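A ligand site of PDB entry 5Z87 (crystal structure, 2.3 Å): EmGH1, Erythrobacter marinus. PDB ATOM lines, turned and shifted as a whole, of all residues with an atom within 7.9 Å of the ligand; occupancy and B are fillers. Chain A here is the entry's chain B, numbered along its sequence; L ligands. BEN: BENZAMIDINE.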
ATOM      1  N   TYR A  36      13.173   9.979   5.438  1.00  0.00           N
ATOM      2  CA  TYR A  36      13.532  10.704   4.211  1.00  0.00           C
ATOM      3  C   TYR A  36      14.449   9.884   3.311  1.00  0.00           C
ATOM      4  O   TYR A  36      14.466  10.115   2.095  1.00  0.00           O
ATOM      5  CB  TYR A  36      14.175  12.057   4.543  1.00  0.00           C
ATOM      6  CG  TYR A  36      15.652  12.030   4.846  1.00  0.00           C
ATOM      7  CD1 TYR A  36      16.594  12.156   3.830  1.00  0.00           C
ATOM      8  CD2 TYR A  36      16.117  11.892   6.147  1.00  0.00           C
ATOM      9  CE1 TYR A  36      17.960  12.129   4.111  1.00  0.00           C
ATOM     10  CE2 TYR A  36      17.466  11.851   6.447  1.00  0.00           C
ATOM     11  CZ  TYR A  36      18.389  11.970   5.419  1.00  0.00           C
ATOM     12  OH  TYR A  36      19.738  11.929   5.719  1.00  0.00           O
ATOM     13  N   ARG A  37      15.171   8.905   3.860  1.00  0.00           N
ATOM     14  CA  ARG A  37      16.027   8.084   3.014  1.00  0.00           C
ATOM     15  C   ARG A  37      15.259   7.004   2.276  1.00  0.00           C
ATOM     16  O   ARG A  37      15.869   6.283   1.476  1.00  0.00           O
ATOM     17  CB  ARG A  37      17.139   7.468   3.858  1.00  0.00           C
ATOM     18  CG  ARG A  37      17.958   8.527   4.581  1.00  0.00           C
ATOM     19  CD  ARG A  37      19.013   7.918   5.511  1.00  0.00           C
ATOM     20  NE  ARG A  37      19.845   6.922   4.835  1.00  0.00           N
ATOM     21  CZ  ARG A  37      21.043   7.172   4.335  1.00  0.00           C
ATOM     22  NH1 ARG A  37      21.547   8.403   4.413  1.00  0.00           N
ATOM     23  NH2 ARG A  37      21.739   6.206   3.746  1.00  0.00           N
ATOM     24  N   GLN A 113      29.663  18.531  -4.785  1.00  0.00           N
ATOM     25  CA  GLN A 113      30.400  17.860  -3.725  1.00  0.00           C
ATOM     26  C   GLN A 113      30.695  18.823  -2.579  1.00  0.00           C
ATOM     27  O   GLN A 113      30.612  18.436  -1.409  1.00  0.00           O
ATOM     28  CB  GLN A 113      31.682  17.253  -4.281  1.00  0.00           C
ATOM     29  CG  GLN A 113      32.600  16.603  -3.254  1.00  0.00           C
ATOM     30  CD  GLN A 113      33.673  15.735  -3.928  1.00  0.00           C
ATOM     31  OE1 GLN A 113      33.353  14.915  -4.806  1.00  0.00           O
ATOM     32  NE2 GLN A 113      34.943  15.921  -3.536  1.00  0.00           N
ATOM     33  N   GLU A 114      30.989  20.086  -2.903  1.00  0.00           N
ATOM     34  CA  GLU A 114      31.223  21.091  -1.863  1.00  0.00           C
ATOM     35  C   GLU A 114      29.956  21.381  -1.093  1.00  0.00           C
ATOM     36  O   GLU A 114      29.996  21.574   0.125  1.00  0.00           O
ATOM     37  CB  GLU A 114      31.784  22.380  -2.453  1.00  0.00           C
ATOM     38  CG  GLU A 114      33.201  22.262  -3.010  1.00  0.00           C
ATOM     39  CD  GLU A 114      34.277  22.213  -1.932  1.00  0.00           C
ATOM     40  OE1 GLU A 114      33.986  22.541  -0.747  1.00  0.00           O
ATOM     41  OE2 GLU A 114      35.417  21.828  -2.262  1.00  0.00           O
ATOM     42  N   VAL A 115      28.807  21.425  -1.776  1.00  0.00           N
ATOM     43  CA  VAL A 115      27.555  21.707  -1.094  1.00  0.00           C
ATOM     44  C   VAL A 115      27.158  20.526  -0.208  1.00  0.00           C
ATOM     45  O   VAL A 115      26.839  20.684   0.975  1.00  0.00           O
ATOM     46  CB  VAL A 115      26.438  22.018  -2.107  1.00  0.00           C
ATOM     47  CG1 VAL A 115      25.111  22.159  -1.382  1.00  0.00           C
ATOM     48  CG2 VAL A 115      26.759  23.256  -2.940  1.00  0.00           C
ATOM     49  N   VAL A 116      27.123  19.327  -0.805  1.00  0.00           N
ATOM     50  CA  VAL A 116      26.708  18.123  -0.102  1.00  0.00           C
ATOM     51  C   VAL A 116      27.609  17.842   1.101  1.00  0.00           C
ATOM     52  O   VAL A 116      27.134  17.363   2.135  1.00  0.00           O
ATOM     53  CB  VAL A 116      26.683  16.949  -1.100  1.00  0.00           C
ATOM     54  CG1 VAL A 116      26.916  15.639  -0.414  1.00  0.00           C
ATOM     55  CG2 VAL A 116      25.362  16.944  -1.849  1.00  0.00           C
ATOM     56  N   SER A 117      28.890  18.173   1.000  1.00  0.00           N
ATOM     57  CA  SER A 117      29.782  17.976   2.142  1.00  0.00           C
ATOM     58  C   SER A 117      29.487  18.933   3.292  1.00  0.00           C
ATOM     59  O   SER A 117      30.000  18.708   4.397  1.00  0.00           O
ATOM     60  CB  SER A 117      31.224  18.149   1.696  1.00  0.00           C
ATOM     61  OG  SER A 117      31.600  19.521   1.771  1.00  0.00           O
ATOM     62  N   ARG A 118      28.697  19.979   3.087  1.00  0.00           N
ATOM     63  CA  ARG A 118      28.439  20.935   4.150  1.00  0.00           C
ATOM     64  C   ARG A 118      27.132  20.672   4.891  1.00  0.00           C
ATOM     65  O   ARG A 118      26.993  21.092   6.050  1.00  0.00           O
ATOM     66  CB  ARG A 118      28.443  22.366   3.587  1.00  0.00           C
ATOM     67  CG  ARG A 118      29.858  22.872   3.346  1.00  0.00           C
ATOM     68  CD  ARG A 118      29.916  24.210   2.588  1.00  0.00           C
ATOM     69  NE  ARG A 118      31.197  24.882   2.786  1.00  0.00           N
ATOM     70  CZ  ARG A 118      32.276  24.649   2.047  1.00  0.00           C
ATOM     71  NH1 ARG A 118      33.405  25.301   2.280  1.00  0.00           N
ATOM     72  NH2 ARG A 118      32.228  23.765   1.065  1.00  0.00           N
ATOM     73  N   SER A 119      26.191  19.982   4.264  1.00  0.00           N
ATOM     74  CA  SER A 119      24.911  19.662   4.868  1.00  0.00           C
ATOM     75  C   SER A 119      24.999  18.360   5.660  1.00  0.00           C
ATOM     76  O   SER A 119      25.476  17.352   5.131  1.00  0.00           O
ATOM     77  CB  SER A 119      23.844  19.534   3.772  1.00  0.00           C
ATOM     78  OG  SER A 119      22.639  18.980   4.264  1.00  0.00           O
ATOM     79  N   ARG A 120      24.531  18.391   6.911  1.00  0.00           N
ATOM     80  CA  ARG A 120      24.439  17.167   7.725  1.00  0.00           C
ATOM     81  C   ARG A 120      23.715  16.045   6.982  1.00  0.00           C
ATOM     82  O   ARG A 120      23.961  14.859   7.235  1.00  0.00           O
ATOM     83  CB  ARG A 120      23.710  17.440   9.040  1.00  0.00           C
ATOM     84  CG  ARG A 120      24.545  17.964  10.180  1.00  0.00           C
ATOM     85  CD  ARG A 120      23.772  17.798  11.504  1.00  0.00           C
ATOM     86  NE  ARG A 120      22.455  18.421  11.464  1.00  0.00           N
ATOM     87  CZ  ARG A 120      21.465  18.145  12.305  1.00  0.00           C
ATOM     88  NH1 ARG A 120      20.297  18.782  12.189  1.00  0.00           N
ATOM     89  NH2 ARG A 120      21.631  17.233  13.253  1.00  0.00           N
ATOM     90  N   PHE A 121      22.814  16.413   6.079  1.00  0.00           N
ATOM     91  CA  PHE A 121      21.980  15.453   5.374  1.00  0.00           C
ATOM     92  C   PHE A 121      22.334  15.357   3.891  1.00  0.00           C
ATOM     93  O   PHE A 121      21.590  14.736   3.132  1.00  0.00           O
ATOM     94  CB  PHE A 121      20.504  15.831   5.571  1.00  0.00           C
ATOM     95  CG  PHE A 121      20.154  16.111   7.002  1.00  0.00           C
ATOM     96  CD1 PHE A 121      19.970  15.057   7.897  1.00  0.00           C
ATOM     97  CD2 PHE A 121      20.052  17.401   7.474  1.00  0.00           C
ATOM     98  CE1 PHE A 121      19.643  15.308   9.230  1.00  0.00           C
ATOM     99  CE2 PHE A 121      19.727  17.666   8.797  1.00  0.00           C
ATOM    100  CZ  PHE A 121      19.529  16.627   9.681  1.00  0.00           C
ATOM    101  N   GLY A 122      23.474  15.926   3.484  1.00  0.00           N
ATOM    102  CA  GLY A 122      23.885  15.893   2.087  1.00  0.00           C
ATOM    103  C   GLY A 122      22.893  16.473   1.093  1.00  0.00           C
ATOM    104  O   GLY A 122      22.720  15.920   0.006  1.00  0.00           O
ATOM    105  N   ILE A 123      22.227  17.572   1.443  1.00  0.00           N
ATOM    106  CA  ILE A 123      21.286  18.209   0.514  1.00  0.00           C
ATOM    107  C   ILE A 123      22.054  18.886  -0.613  1.00  0.00           C
ATOM    108  O   ILE A 123      22.831  19.828  -0.346  1.00  0.00           O
ATOM    109  CB  ILE A 123      20.387  19.240   1.223  1.00  0.00           C
ATOM    110  CG1 ILE A 123      19.721  18.621   2.471  1.00  0.00           C
ATOM    111  CG2 ILE A 123      19.331  19.799   0.234  1.00  0.00           C
ATOM    112  CD1 ILE A 123      19.138  19.654   3.441  1.00  0.00           C
ATOM    113  N   PHE A 386      18.651  13.753  -4.385  1.00  0.00           N
ATOM    114  CA  PHE A 386      19.180  12.919  -3.303  1.00  0.00           C
ATOM    115  C   PHE A 386      19.581  11.530  -3.776  1.00  0.00           C
ATOM    116  O   PHE A 386      20.367  10.870  -3.083  1.00  0.00           O
ATOM    117  CB  PHE A 386      18.149  12.773  -2.175  1.00  0.00           C
ATOM    118  CG  PHE A 386      17.944  14.010  -1.370  1.00  0.00           C
ATOM    119  CD1 PHE A 386      18.718  14.259  -0.253  1.00  0.00           C
ATOM    120  CD2 PHE A 386      16.984  14.941  -1.731  1.00  0.00           C
ATOM    121  CE1 PHE A 386      18.517  15.396   0.502  1.00  0.00           C
ATOM    122  CE2 PHE A 386      16.770  16.064  -0.986  1.00  0.00           C
ATOM    123  CZ  PHE A 386      17.551  16.306   0.131  1.00  0.00           C
ATOM    124  N   PHE A 390      25.278  13.925  -9.870  1.00  0.00           N
ATOM    125  CA  PHE A 390      25.064  15.359 -10.093  1.00  0.00           C
ATOM    126  C   PHE A 390      24.943  15.708 -11.574  1.00  0.00           C
ATOM    127  O   PHE A 390      24.203  16.632 -11.933  1.00  0.00           O
ATOM    128  CB  PHE A 390      26.205  16.162  -9.467  1.00  0.00           C
ATOM    129  CG  PHE A 390      26.428  15.870  -8.007  1.00  0.00           C
ATOM    130  CD1 PHE A 390      25.362  15.863  -7.115  1.00  0.00           C
ATOM    131  CD2 PHE A 390      27.696  15.597  -7.532  1.00  0.00           C
ATOM    132  CE1 PHE A 390      25.574  15.605  -5.766  1.00  0.00           C
ATOM    133  CE2 PHE A 390      27.909  15.338  -6.194  1.00  0.00           C
ATOM    134  CZ  PHE A 390      26.838  15.339  -5.312  1.00  0.00           C
HETATM  135  C1  BEN L   1      26.678  14.083   4.086  1.00  0.00           C
HETATM  136  C2  BEN L   1      25.498  13.557   4.610  1.00  0.00           C
HETATM  137  C3  BEN L   1      24.721  12.717   3.829  1.00  0.00           C
HETATM  138  C4  BEN L   1      25.129  12.410   2.534  1.00  0.00           C
HETATM  139  C5  BEN L   1      26.308  12.950   2.010  1.00  0.00           C
HETATM  140  C6  BEN L   1      27.093  13.797   2.792  1.00  0.00           C
HETATM  141  C   BEN L   1      27.500  15.001   4.921  1.00  0.00           C
HETATM  142  N1  BEN L   1      28.259  15.894   4.333  1.00  0.00           N
HETATM  143  N2  BEN L   1      27.472  14.913   6.255  1.00  0.00           N
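OG of Ser 119 sits at hydrogen-bond distance from N of Gly 122 (3.3 Å). The side-chain hydroxyl (OG) of Ser 119 sits close to the backbone NH (N) of Phe 121, at 3.1 Å. The backbone NH (N) of Ile 123 sits at hydrogen-bond distance from the side-chain hydroxyl (OG) of Ser 119. O of Glu 114 sits at hydrogen-bond distance from OG of Ser 117 (3.1 Å).
N1 of the ligand lies within hydrogen-bond range of O of Val 116 (2.9 Å). The backbone carbonyl oxygen of Ser 119 lies close to a nitrogen (N1) of the ligand (3.2 Å). O of Ser 117 is in hydrogen-bond range of N1 of the ligand (3.3 Å).
Arg 120 touches the ligand (O to C2, 3.3 Å). C of Phe 121 touches C3 of the ligand (3.6 Å). Gly 122 touches the ligand. Hydrophobic or aromatic side chains within 4 Å of the ligand: Val 116. The nearest printed residue that does not touch the ligand is Arg 118 (4.3 Å).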
